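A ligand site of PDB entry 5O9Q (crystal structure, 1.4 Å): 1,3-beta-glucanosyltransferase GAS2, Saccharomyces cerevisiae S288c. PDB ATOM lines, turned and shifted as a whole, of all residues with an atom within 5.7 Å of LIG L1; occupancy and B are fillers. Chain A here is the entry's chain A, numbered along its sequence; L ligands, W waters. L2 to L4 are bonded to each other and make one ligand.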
ATOM      1  N   GLN A  60      21.971  -9.861   4.996  1.00  0.00           N
ATOM      2  CA  GLN A  60      20.889 -10.741   5.444  1.00  0.00           C
ATOM      3  C   GLN A  60      20.010 -10.003   6.440  1.00  0.00           C
ATOM      4  O   GLN A  60      20.500  -9.514   7.459  1.00  0.00           O
ATOM      5  CB  GLN A  60      21.436 -12.016   6.089  1.00  0.00           C
ATOM      6  CG  GLN A  60      20.387 -13.098   6.333  1.00  0.00           C
ATOM      7  CD  GLN A  60      19.940 -13.791   5.069  1.00  0.00           C
ATOM      8  OE1 GLN A  60      20.766 -14.209   4.264  1.00  0.00           O
ATOM      9  NE2 GLN A  60      18.630 -13.936   4.882  1.00  0.00           N
ATOM     10  N   GLN A  62      16.730  -9.914   9.117  1.00  0.00           N
ATOM     11  CA  GLN A  62      16.027 -10.787  10.060  1.00  0.00           C
ATOM     12  C   GLN A  62      14.612 -10.263  10.315  1.00  0.00           C
ATOM     13  O   GLN A  62      14.313  -9.099  10.023  1.00  0.00           O
ATOM     14  CB  GLN A  62      16.801 -10.904  11.384  1.00  0.00           C
ATOM     15  CG  GLN A  62      16.485  -9.850  12.447  1.00  0.00           C
ATOM     16  CD  GLN A  62      17.358  -9.941  13.684  1.00  0.00           C
ATOM     17  OE1 GLN A  62      18.450 -10.516  13.653  1.00  0.00           O
ATOM     18  NE2 GLN A  62      16.893  -9.358  14.780  1.00  0.00           N
ATOM     19  N   TYR A 107      22.951 -15.796   3.906  1.00  0.00           N
ATOM     20  CA  TYR A 107      22.762 -16.995   4.730  1.00  0.00           C
ATOM     21  C   TYR A 107      21.505 -17.775   4.373  1.00  0.00           C
ATOM     22  O   TYR A 107      21.424 -18.958   4.686  1.00  0.00           O
ATOM     23  CB  TYR A 107      22.719 -16.623   6.213  1.00  0.00           C
ATOM     24  CG  TYR A 107      24.014 -16.046   6.730  1.00  0.00           C
ATOM     25  CD1 TYR A 107      24.331 -14.708   6.546  1.00  0.00           C
ATOM     26  CD2 TYR A 107      24.936 -16.851   7.413  1.00  0.00           C
ATOM     27  CE1 TYR A 107      25.512 -14.170   7.024  1.00  0.00           C
ATOM     28  CE2 TYR A 107      26.124 -16.319   7.895  1.00  0.00           C
ATOM     29  CZ  TYR A 107      26.410 -14.980   7.688  1.00  0.00           C
ATOM     30  OH  TYR A 107      27.585 -14.436   8.161  1.00  0.00           O
ATOM     31  N   ALA A 108      20.532 -17.146   3.729  1.00  0.00           N
ATOM     32  CA  ALA A 108      19.289 -17.831   3.390  1.00  0.00           C
ATOM     33  C   ALA A 108      18.557 -17.166   2.246  1.00  0.00           C
ATOM     34  O   ALA A 108      18.333 -15.949   2.267  1.00  0.00           O
ATOM     35  CB  ALA A 108      18.382 -17.919   4.613  1.00  0.00           C
ATOM     36  N   ASP A 132      24.916 -19.734   1.719  1.00  0.00           N
ATOM     37  CA  ASP A 132      24.645 -20.935   2.505  1.00  0.00           C
ATOM     38  C   ASP A 132      23.481 -21.706   1.870  1.00  0.00           C
ATOM     39  O   ASP A 132      22.528 -21.102   1.386  1.00  0.00           O
ATOM     40  CB  ASP A 132      24.306 -20.576   3.959  1.00  0.00           C
ATOM     41  CG  ASP A 132      25.478 -19.945   4.684  1.00  0.00           C
ATOM     42  OD1 ASP A 132      25.763 -18.754   4.438  1.00  0.00           O
ATOM     43  OD2 ASP A 132      26.123 -20.633   5.503  1.00  0.00           O
ATOM     44  N   SER A 134      21.774 -24.043   3.654  1.00  0.00           N
ATOM     45  CA  SER A 134      20.863 -24.320   4.764  1.00  0.00           C
ATOM     46  C   SER A 134      20.077 -23.085   5.182  1.00  0.00           C
ATOM     47  O   SER A 134      20.339 -21.974   4.709  1.00  0.00           O
ATOM     48  CB  SER A 134      21.681 -24.842   5.951  1.00  0.00           C
ATOM     49  OG  SER A 134      22.663 -23.892   6.336  1.00  0.00           O
ATOM     50  N   GLU A 135      19.113 -23.291   6.066  1.00  0.00           N
ATOM     51  CA  GLU A 135      18.384 -22.201   6.696  1.00  0.00           C
ATOM     52  C   GLU A 135      18.077 -22.633   8.135  1.00  0.00           C
ATOM     53  O   GLU A 135      18.195 -23.826   8.433  1.00  0.00           O
ATOM     54  CB  GLU A 135      17.122 -21.833   5.882  1.00  0.00           C
ATOM     55  CG  GLU A 135      16.105 -22.960   5.687  1.00  0.00           C
ATOM     56  CD  GLU A 135      14.864 -22.833   6.555  1.00  0.00           C
ATOM     57  OE1 GLU A 135      14.939 -22.225   7.651  1.00  0.00           O
ATOM     58  OE2 GLU A 135      13.811 -23.354   6.136  1.00  0.00           O
ATOM     59  N   PRO A 136      17.722 -21.694   9.036  1.00  0.00           N
ATOM     60  CA  PRO A 136      17.632 -22.050  10.459  1.00  0.00           C
ATOM     61  C   PRO A 136      16.771 -23.263  10.807  1.00  0.00           C
ATOM     62  O   PRO A 136      17.120 -24.015  11.729  1.00  0.00           O
ATOM     63  CB  PRO A 136      17.064 -20.779  11.094  1.00  0.00           C
ATOM     64  CG  PRO A 136      17.514 -19.684  10.195  1.00  0.00           C
ATOM     65  CD  PRO A 136      17.419 -20.265   8.812  1.00  0.00           C
ATOM     66  N   ASP A 137      15.668 -23.449  10.088  1.00  0.00           N
ATOM     67  CA  ASP A 137      14.765 -24.589  10.305  1.00  0.00           C
ATOM     68  C   ASP A 137      15.054 -25.829   9.454  1.00  0.00           C
ATOM     69  O   ASP A 137      14.458 -26.878   9.679  1.00  0.00           O
ATOM     70  CB  ASP A 137      13.305 -24.153  10.092  1.00  0.00           C
ATOM     71  CG  ASP A 137      12.868 -23.051  11.062  1.00  0.00           C
ATOM     72  OD1 ASP A 137      13.410 -22.959  12.186  1.00  0.00           O
ATOM     73  OD2 ASP A 137      11.968 -22.270  10.692  1.00  0.00           O
ATOM     74  N   ILE A 138      15.971 -25.725   8.481  1.00  0.00           N
ATOM     75  CA  ILE A 138      16.455 -26.881   7.723  1.00  0.00           C
ATOM     76  C   ILE A 138      17.980 -26.826   7.633  1.00  0.00           C
ATOM     77  O   ILE A 138      18.550 -26.326   6.653  1.00  0.00           O
ATOM     78  CB  ILE A 138      15.814 -27.002   6.308  1.00  0.00           C
ATOM     79  CG1 ILE A 138      14.277 -26.871   6.375  1.00  0.00           C
ATOM     80  CG2 ILE A 138      16.202 -28.338   5.672  1.00  0.00           C
ATOM     81  CD1 ILE A 138      13.608 -26.860   5.022  1.00  0.00           C
ATOM     82  N   SER A 139      18.622 -27.323   8.689  1.00  0.00           N
ATOM     83  CA  SER A 139      20.074 -27.416   8.797  1.00  0.00           C
ATOM     84  C   SER A 139      20.434 -28.747   9.420  1.00  0.00           C
ATOM     85  O   SER A 139      19.571 -29.399  10.028  1.00  0.00           O
ATOM     86  CB  SER A 139      20.627 -26.317   9.695  1.00  0.00           C
ATOM     87  OG  SER A 139      20.457 -25.030   9.134  1.00  0.00           O
ATOM     88  N   ILE A 140      21.691 -29.132   9.314  1.00  0.00           N
ATOM     89  CA  ILE A 140      22.205 -30.279  10.067  1.00  0.00           C
ATOM     90  C   ILE A 140      22.203 -29.866  11.546  1.00  0.00           C
ATOM     91  O   ILE A 140      22.871 -28.911  11.930  1.00  0.00           O
ATOM     92  CB  ILE A 140      23.598 -30.712   9.589  1.00  0.00           C
ATOM     93  CG1 ILE A 140      23.517 -31.221   8.148  1.00  0.00           C
ATOM     94  CG2 ILE A 140      24.165 -31.800  10.499  1.00  0.00           C
ATOM     95  CD1 ILE A 140      24.849 -31.328   7.440  1.00  0.00           C
ATOM     96  N   ASN A 141      21.427 -30.592  12.349  1.00  0.00           N
ATOM     97  CA  ASN A 141      21.244 -30.278  13.761  1.00  0.00           C
ATOM     98  C   ASN A 141      22.482 -30.738  14.528  1.00  0.00           C
ATOM     99  O   ASN A 141      22.685 -31.930  14.683  1.00  0.00           O
ATOM    100  CB  ASN A 141      19.988 -30.994  14.280  1.00  0.00           C
ATOM    101  CG  ASN A 141      19.629 -30.617  15.722  1.00  0.00           C
ATOM    102  OD1 ASN A 141      20.389 -29.954  16.424  1.00  0.00           O
ATOM    103  ND2 ASN A 141      18.456 -31.057  16.156  1.00  0.00           N
ATOM    104  N   ARG A 142      23.283 -29.800  15.029  1.00  0.00           N
ATOM    105  CA  ARG A 142      24.509 -30.178  15.748  1.00  0.00           C
ATOM    106  C   ARG A 142      24.233 -30.959  17.055  1.00  0.00           C
ATOM    107  O   ARG A 142      25.107 -31.706  17.509  1.00  0.00           O
ATOM    108  CB  ARG A 142      25.394 -28.951  16.025  1.00  0.00           C
ATOM    109  CG  ARG A 142      24.860 -27.953  17.043  1.00  0.00           C
ATOM    110  CD  ARG A 142      25.884 -26.882  17.374  1.00  0.00           C
ATOM    111  NE  ARG A 142      26.079 -25.901  16.297  1.00  0.00           N
ATOM    112  CZ  ARG A 142      25.334 -24.799  16.106  1.00  0.00           C
ATOM    113  NH1 ARG A 142      24.306 -24.492  16.902  1.00  0.00           N
ATOM    114  NH2 ARG A 142      25.631 -23.984  15.100  1.00  0.00           N
ATOM    115  N   GLU A 143      23.038 -30.791  17.623  1.00  0.00           N
ATOM    116  CA  GLU A 143      22.598 -31.526  18.832  1.00  0.00           C
ATOM    117  C   GLU A 143      22.033 -32.928  18.565  1.00  0.00           C
ATOM    118  O   GLU A 143      21.843 -33.708  19.504  1.00  0.00           O
ATOM    119  CB  GLU A 143      21.514 -30.716  19.561  1.00  0.00           C
ATOM    120  CG  GLU A 143      21.884 -29.273  19.924  1.00  0.00           C
ATOM    121  CD  GLU A 143      23.078 -29.185  20.845  1.00  0.00           C
ATOM    122  OE1 GLU A 143      23.195 -30.017  21.776  1.00  0.00           O
ATOM    123  OE2 GLU A 143      23.902 -28.260  20.654  1.00  0.00           O
ATOM    124  N   ASN A 175      27.326 -24.209   8.390  1.00  0.00           N
ATOM    125  CA  ASN A 175      27.894 -23.087   9.121  1.00  0.00           C
ATOM    126  C   ASN A 175      28.018 -23.464  10.580  1.00  0.00           C
ATOM    127  O   ASN A 175      27.009 -23.656  11.263  1.00  0.00           O
ATOM    128  CB  ASN A 175      27.042 -21.831   8.957  1.00  0.00           C
ATOM    129  CG  ASN A 175      27.669 -20.615   9.616  1.00  0.00           C
ATOM    130  OD1 ASN A 175      28.763 -20.196   9.245  1.00  0.00           O
ATOM    131  ND2 ASN A 175      26.988 -20.051  10.603  1.00  0.00           N
ATOM    132  N   GLU A 176      29.255 -23.611  11.061  1.00  0.00           N
ATOM    133  CA  GLU A 176      29.524 -23.860  12.481  1.00  0.00           C
ATOM    134  C   GLU A 176      28.692 -24.995  13.043  1.00  0.00           C
ATOM    135  O   GLU A 176      28.029 -24.838  14.081  1.00  0.00           O
ATOM    136  CB  GLU A 176      29.266 -22.583  13.290  1.00  0.00           C
ATOM    137  CG  GLU A 176      30.010 -21.373  12.757  1.00  0.00           C
ATOM    138  CD  GLU A 176      29.872 -20.151  13.652  1.00  0.00           C
ATOM    139  OE1 GLU A 176      28.983 -20.115  14.528  1.00  0.00           O
ATOM    140  OE2 GLU A 176      30.674 -19.229  13.468  1.00  0.00           O
ATOM    141  N   VAL A 177      28.690 -26.130  12.356  1.00  0.00           N
ATOM    142  CA  VAL A 177      27.858 -27.259  12.773  1.00  0.00           C
ATOM    143  C   VAL A 177      28.515 -27.828  14.020  1.00  0.00           C
ATOM    144  O   VAL A 177      28.023 -27.610  15.135  1.00  0.00           O
ATOM    145  CB  VAL A 177      27.637 -28.281  11.627  1.00  0.00           C
ATOM    146  CG1 VAL A 177      26.697 -29.384  12.081  1.00  0.00           C
ATOM    147  CG2 VAL A 177      27.083 -27.588  10.394  1.00  0.00           C
ATOM    148  N   TYR A 244      37.008 -13.521  14.624  1.00  0.00           N
ATOM    149  CA  TYR A 244      36.783 -12.338  15.462  1.00  0.00           C
ATOM    150  C   TYR A 244      37.936 -12.053  16.439  1.00  0.00           C
ATOM    151  O   TYR A 244      37.746 -11.355  17.442  1.00  0.00           O
ATOM    152  CB  TYR A 244      35.467 -12.497  16.213  1.00  0.00           C
ATOM    153  CG  TYR A 244      34.261 -12.469  15.309  1.00  0.00           C
ATOM    154  CD1 TYR A 244      33.800 -13.641  14.688  1.00  0.00           C
ATOM    155  CD2 TYR A 244      33.594 -11.282  15.050  1.00  0.00           C
ATOM    156  CE1 TYR A 244      32.691 -13.610  13.847  1.00  0.00           C
ATOM    157  CE2 TYR A 244      32.487 -11.244  14.215  1.00  0.00           C
ATOM    158  CZ  TYR A 244      32.043 -12.407  13.625  1.00  0.00           C
ATOM    159  OH  TYR A 244      30.939 -12.345  12.795  1.00  0.00           O
ATOM    160  N   GLU A 275      33.420 -14.524   8.023  1.00  0.00           N
ATOM    161  CA  GLU A 275      32.979 -13.370   8.803  1.00  0.00           C
ATOM    162  C   GLU A 275      34.204 -12.740   9.450  1.00  0.00           C
ATOM    163  O   GLU A 275      35.144 -13.443   9.822  1.00  0.00           O
ATOM    164  CB  GLU A 275      32.007 -13.781   9.913  1.00  0.00           C
ATOM    165  CG  GLU A 275      30.643 -14.257   9.453  1.00  0.00           C
ATOM    166  CD  GLU A 275      29.799 -14.828  10.582  1.00  0.00           C
ATOM    167  OE1 GLU A 275      30.170 -14.699  11.759  1.00  0.00           O
ATOM    168  OE2 GLU A 275      28.737 -15.407  10.275  1.00  0.00           O
ATOM    169  N   TYR A 307      31.115  -8.678   8.931  1.00  0.00           N
ATOM    170  CA  TYR A 307      29.787  -8.946   9.468  1.00  0.00           C
ATOM    171  C   TYR A 307      29.315  -7.698  10.220  1.00  0.00           C
ATOM    172  O   TYR A 307      29.928  -7.351  11.225  1.00  0.00           O
ATOM    173  CB  TYR A 307      29.817 -10.159  10.418  1.00  0.00           C
ATOM    174  CG  TYR A 307      28.432 -10.541  10.864  1.00  0.00           C
ATOM    175  CD1 TYR A 307      27.867  -9.978  12.012  1.00  0.00           C
ATOM    176  CD2 TYR A 307      27.660 -11.426  10.125  1.00  0.00           C
ATOM    177  CE1 TYR A 307      26.580 -10.303  12.413  1.00  0.00           C
ATOM    178  CE2 TYR A 307      26.365 -11.752  10.515  1.00  0.00           C
ATOM    179  CZ  TYR A 307      25.828 -11.193  11.661  1.00  0.00           C
ATOM    180  OH  TYR A 307      24.563 -11.515  12.056  1.00  0.00           O
ATOM    181  N   MET A 308      28.265  -6.986   9.776  1.00  0.00           N
ATOM    182  CA  MET A 308      27.541  -7.202   8.511  1.00  0.00           C
ATOM    183  C   MET A 308      26.976  -5.858   8.026  1.00  0.00           C
ATOM    184  O   MET A 308      27.217  -4.829   8.644  1.00  0.00           O
ATOM    185  CB  MET A 308      26.423  -8.237   8.695  1.00  0.00           C
ATOM    186  CG  MET A 308      25.180  -7.762   9.453  1.00  0.00           C
ATOM    187  SD  MET A 308      23.606  -8.414   8.866  1.00  0.00           S
ATOM    188  CE  MET A 308      23.705  -8.212   7.114  1.00  0.00           C
ATOM    189  N   GLU A 312      21.018  -4.736  13.533  1.00  0.00           N
ATOM    190  CA  GLU A 312      19.849  -5.450  14.063  1.00  0.00           C
ATOM    191  C   GLU A 312      19.925  -5.581  15.588  1.00  0.00           C
ATOM    192  O   GLU A 312      19.912  -6.683  16.131  1.00  0.00           O
ATOM    193  CB  GLU A 312      19.730  -6.825  13.405  1.00  0.00           C
ATOM    194  CG  GLU A 312      19.552  -6.761  11.894  1.00  0.00           C
ATOM    195  CD  GLU A 312      19.394  -8.119  11.269  1.00  0.00           C
ATOM    196  OE1 GLU A 312      18.479  -8.290  10.430  1.00  0.00           O
ATOM    197  OE2 GLU A 312      20.174  -9.037  11.611  1.00  0.00           O
ATOM    198  N   TYR A 316      26.489  -4.737  15.075  1.00  0.00           N
ATOM    199  CA  TYR A 316      27.299  -5.305  13.984  1.00  0.00           C
ATOM    200  C   TYR A 316      27.035  -4.683  12.611  1.00  0.00           C
ATOM    201  O   TYR A 316      27.743  -5.009  11.656  1.00  0.00           O
ATOM    202  CB  TYR A 316      27.129  -6.827  13.911  1.00  0.00           C
ATOM    203  CG  TYR A 316      27.888  -7.573  14.974  1.00  0.00           C
ATOM    204  CD1 TYR A 316      29.280  -7.676  14.935  1.00  0.00           C
ATOM    205  CD2 TYR A 316      27.222  -8.177  16.044  1.00  0.00           C
ATOM    206  CE1 TYR A 316      29.986  -8.347  15.908  1.00  0.00           C
ATOM    207  CE2 TYR A 316      27.921  -8.863  17.032  1.00  0.00           C
ATOM    208  CZ  TYR A 316      29.300  -8.940  16.957  1.00  0.00           C
ATOM    209  OH  TYR A 316      29.993  -9.613  17.949  1.00  0.00           O
HETATM  210  C1  LIG L   1      21.865 -26.110  13.600  1.00  0.00           C
HETATM  211  C2  LIG L   1      22.951 -25.143  13.151  1.00  0.00           C
HETATM  212  C3  LIG L   1      24.200 -25.865  12.587  1.00  0.00           C
HETATM  213  C4  LIG L   1      20.634 -25.323  14.070  1.00  0.00           C
HETATM  214  C5  LIG L   1      29.641 -13.365  18.933  1.00  0.00           C
HETATM  215  C6  LIG L   1      30.306 -14.161  19.866  1.00  0.00           C
HETATM  216  C7  LIG L   1      31.402 -14.929  19.486  1.00  0.00           C
HETATM  217  C8  LIG L   1      31.839 -14.895  18.168  1.00  0.00           C
HETATM  218  C9  LIG L   1      31.180 -14.095  17.229  1.00  0.00           C
HETATM  219  C10 LIG L   1      30.077 -13.328  17.597  1.00  0.00           C
HETATM  220  C11 LIG L   1      29.430 -12.543  16.644  1.00  0.00           C
HETATM  221  O1  LIG L   1      28.657 -13.389  15.783  1.00  0.00           O
HETATM  222  C12 LIG L   1      27.997 -12.663  14.748  1.00  0.00           C
HETATM  223  C13 LIG L   1      26.855 -13.509  14.181  1.00  0.00           C
HETATM  224  C14 LIG L   1      26.773 -14.007  12.954  1.00  0.00           C
HETATM  225  N1  LIG L   1      25.764 -13.869  14.846  1.00  0.00           N
HETATM  226  N2  LIG L   1      25.065 -14.526  14.084  1.00  0.00           N
HETATM  227  N3  LIG L   1      25.618 -14.661  12.948  1.00  0.00           N
HETATM  228  C15 LIG L   1      25.020 -15.363  11.804  1.00  0.00           C
HETATM  229  C16 LIG L   1      24.222 -16.596  12.187  1.00  0.00           C
HETATM  230  O2  LIG L   1      25.121 -17.642  12.560  1.00  0.00           O
HETATM  231  O3  LIG L   1      24.145 -14.345  11.313  1.00  0.00           O
HETATM  232  C17 LIG L   1      23.437 -14.743  10.136  1.00  0.00           C
HETATM  233  C18 LIG L   1      22.657 -13.535   9.585  1.00  0.00           C
HETATM  234  O4  LIG L   1      22.269 -12.689  10.651  1.00  0.00           O
HETATM  235  C19 LIG L   1      22.519 -15.901  10.485  1.00  0.00           C
HETATM  236  O5  LIG L   1      21.799 -16.338   9.319  1.00  0.00           O
HETATM  237  C20 LIG L   1      23.368 -17.059  11.002  1.00  0.00           C
HETATM  238  O6  LIG L   1      22.466 -18.081  11.441  1.00  0.00           O
HETATM  239  C21 LIG L   1      22.752 -19.384  10.932  1.00  0.00           C
HETATM  240  C22 LIG L   1      21.763 -20.344  11.579  1.00  0.00           C
HETATM  241  O7  LIG L   1      21.965 -20.349  13.001  1.00  0.00           O
HETATM  242  O8  LIG L   1      22.537 -19.371   9.518  1.00  0.00           O
HETATM  243  C23 LIG L   1      22.813 -20.641   8.909  1.00  0.00           C
HETATM  244  C24 LIG L   1      22.611 -20.449   7.405  1.00  0.00           C
HETATM  245  O9  LIG L   1      21.255 -20.060   7.133  1.00  0.00           O
HETATM  246  C25 LIG L   1      21.870 -21.708   9.481  1.00  0.00           C
HETATM  247  O10 LIG L   1      22.236 -22.989   8.950  1.00  0.00           O
HETATM  248  C26 LIG L   1      21.966 -21.743  10.995  1.00  0.00           C
HETATM  249  O11 LIG L   1      20.945 -22.616  11.495  1.00  0.00           O
HETATM  250  C27 LIG L   1      21.367 -23.477  12.565  1.00  0.00           C
HETATM  251  O12 LIG L   1      22.423 -24.336  12.098  1.00  0.00           O
HETATM  252  O13 LIG L   1      23.873 -26.532  11.359  1.00  0.00           O
HETATM  253  O14 LIG L   1      22.338 -26.916  14.690  1.00  0.00           O
HETATM  254  O15 LIG L   1      19.564 -26.246  14.333  1.00  0.00           O
HETATM  255  C28 LIG L   1      20.195 -24.329  13.003  1.00  0.00           C
HETATM  256  O16 LIG L   1      19.161 -23.502  13.551  1.00  0.00           O
HETATM  257  C1  LG2 L   2      39.963 -11.305  21.593  1.00  0.00           C
HETATM  258  C2  LG2 L   2      40.596 -12.688  21.487  1.00  0.00           C
HETATM  259  C3  LG2 L   2      42.085 -12.581  21.143  1.00  0.00           C
HETATM  260  C4  LG2 L   2      42.805 -11.559  22.027  1.00  0.00           C
HETATM  261  C5  LG2 L   2      44.231 -11.331  21.539  1.00  0.00           C
HETATM  262  C6  LG2 L   2      40.768 -10.415  22.531  1.00  0.00           C
HETATM  263  O1  LG2 L   2      40.180  -9.108  22.604  1.00  0.00           O
HETATM  264  O2  LG2 L   2      38.617 -11.411  22.061  1.00  0.00           O
HETATM  265  O3  LG2 L   2      39.897 -13.450  20.475  1.00  0.00           O
HETATM  266  O4  LG2 L   2      42.712 -13.856  21.299  1.00  0.00           O
HETATM  267  O5  LG2 L   2      42.104 -10.314  22.027  1.00  0.00           O
HETATM  268  O6  LG2 L   2      44.836 -10.242  22.239  1.00  0.00           O
HETATM  269  C1  LG3 L   3      38.539 -15.377  19.980  1.00  0.00           C
HETATM  270  C2  LG3 L   3      38.394 -16.896  20.095  1.00  0.00           C
HETATM  271  C3  LG3 L   3      39.727 -17.588  19.822  1.00  0.00           C
HETATM  272  C4  LG3 L   3      40.817 -17.001  20.717  1.00  0.00           C
HETATM  273  C5  LG3 L   3      42.178 -17.657  20.474  1.00  0.00           C
HETATM  274  C6  LG3 L   3      39.743 -14.855  20.777  1.00  0.00           C
HETATM  275  O1  LG3 L   3      37.344 -14.747  20.454  1.00  0.00           O
HETATM  276  O2  LG3 L   3      37.418 -17.354  19.138  1.00  0.00           O
HETATM  277  O3  LG3 L   3      39.584 -18.992  20.065  1.00  0.00           O
HETATM  278  O4  LG3 L   3      40.915 -15.601  20.446  1.00  0.00           O
HETATM  279  O5  LG3 L   3      42.634 -17.380  19.143  1.00  0.00           O
HETATM  280  C1  LG4 L   4      35.181 -18.087  18.656  1.00  0.00           C
HETATM  281  C2  LG4 L   4      33.867 -18.628  19.229  1.00  0.00           C
HETATM  282  C3  LG4 L   4      34.098 -19.686  20.314  1.00  0.00           C
HETATM  283  C4  LG4 L   4      35.136 -19.215  21.330  1.00  0.00           C
HETATM  284  C5  LG4 L   4      35.468 -20.290  22.355  1.00  0.00           C
HETATM  285  C6  LG4 L   4      36.178 -17.743  19.761  1.00  0.00           C
HETATM  286  O1  LG4 L   4      34.957 -16.933  17.842  1.00  0.00           O
HETATM  287  O2  LG4 L   4      33.104 -19.212  18.171  1.00  0.00           O
HETATM  288  O3  LG4 L   4      32.852 -19.966  20.957  1.00  0.00           O
HETATM  289  O4  LG4 L   4      36.330 -18.867  20.630  1.00  0.00           O
HETATM  290  O5  LG4 L   4      36.410 -19.755  23.287  1.00  0.00           O
HETATM  291  O   HOH W   1      18.811 -28.345  12.951  1.00  0.00           O
HETATM  292  O   HOH W   2      27.498 -17.582  14.727  1.00  0.00           O
HETATM  293  O   HOH W   3      24.474 -25.122   9.092  1.00  0.00           O
HETATM  294  O   HOH W   4      27.935 -17.568  11.817  1.00  0.00           O
HETATM  295  O   HOH W   5      29.618 -15.568  14.321  1.00  0.00           O
HETATM  296  O   HOH W   6      25.179 -21.722  12.117  1.00  0.00           O
HETATM  297  O   HOH W   7      19.960 -18.180   8.595  1.00  0.00           O
HETATM  298  O   HOH W   8      20.417 -11.123   9.749  1.00  0.00           O
HETATM  299  O   HOH W   9      19.407 -15.443   8.351  1.00  0.00           O
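The backbone NH (N) of Ala 108 is in hydrogen-bond range of the side-chain amide oxygen (OE1) of Gln 60, at 3.0 Å.
OH of Tyr 244 sits at hydrogen-bond distance from OE1 of Glu 275, at 2.7 Å.
O of Tyr 316 is in hydrogen-bond range of N of Met 308 (2.8 Å).
The side-chain hydroxyl (OH) of Tyr 107 is in hydrogen-bond range of the side-chain carboxylate (OE2) of Glu 275 (2.6 Å).
The backbone NH (N) of Tyr 107 lies within hydrogen-bond range of the side-chain amide oxygen (OE1) of Gln 60 (2.7 Å).
The backbone NH of Glu 143 is in hydrogen-bond range of the side-chain amide oxygen of Asn 141.
The side-chain hydroxyl (OG) of Ser 139 is in hydrogen-bond range of the backbone carbonyl oxygen (O) of Glu 135 (2.7 Å).
The side-chain carboxylate (OE1) of Glu 135 lies within hydrogen-bond range of the backbone NH (N) of Asp 137 (2.8 Å).
CG of Gln 60 touches C18 of LIG L1, 3.99 Å away.
Asp 132 touches LIG L1 (CB to C24, 3.8 Å).
Glu 135 touches LIG L1.
CA of Asn 141 touches O14 of LIG L1 (3.7 Å).
Asn 175 touches LIG L1 (ND2 to O2, 3.6 Å).
CG2 of Val 177 touches O13 of LIG L1 (3.5 Å).
Tyr 244 touches LIG L1 (OH to C12, 3.5 Å).
Glu 275 touches LIG L1 (OE2 to C14, 3.6 Å).
Tyr 316 touches LIG L1 (OH to C11, 3.3 Å).
Hydrophobic or aromatic side chains within 4 Å of LIG L1: Tyr 107, Val 177, Tyr 244, Tyr 307 and Tyr 316.
Of the 24 residues printed, 16 come within 4 Å of LIG L1.
The backbone carbonyl oxygen (O) of Ser 134 lies within hydrogen-bond range of an oxygen (O9) of LIG L1, at 3.2 Å.
The backbone carbonyl oxygen (O) of Pro 136 sits at hydrogen-bond distance from an oxygen (O16) of LIG L1 (2.8 Å).
The backbone NH (N) of Arg 142 lies within hydrogen-bond range of an oxygen (O14) of LIG L1, at 3.1 Å.
An oxygen (O10) of LIG L1 lies within hydrogen-bond range of the side-chain hydroxyl of Ser 134, at 2.8 Å.
O of Tyr 107 lies within hydrogen-bond range of O9 of LIG L1 (2.7 Å).
An oxygen (O13) of LIG L1 sits at hydrogen-bond distance from the backbone carbonyl oxygen (O) of Ile 140 (2.6 Å).
OH of Tyr 307 is in hydrogen-bond range of O4 of LIG L1 (2.9 Å).
The side-chain hydroxyl of Ser 139 lies within hydrogen-bond range of an oxygen (O10) of LIG L1.
Water W8 lies within hydrogen-bond range of an oxygen (O4) of LIG L1 (2.6 Å), the backbone carbonyl oxygen (O) of Gln 60 (2.8 Å) and the side-chain carboxylate (OE2) of Glu 312 (2.8 Å).
Water W1 bridges an oxygen (O15) of LIG L1 and the backbone carbonyl oxygen (O) of Ser 139.
Water W3 bridges O13 of LIG L1 (2.7 Å) and N of Asn 175 (3.1 Å).
Water W5 bridges OE1 of Glu 275 (2.8 Å) and O1 of LIG L1 (2.8 Å).
Water W4 lies within hydrogen-bond range of the side-chain carboxylate (OE2) of Glu 275 (2.8 Å), an oxygen (O2) of LIG L1 (2.9 Å) and the side-chain amide nitrogen (ND2) of Asn 175 (2.9 Å).
Water W2 lies within hydrogen-bond range of the side-chain carboxylate of Glu 176 (2.9 Å) and an oxygen (O2) of LIG L1 (3.2 Å).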
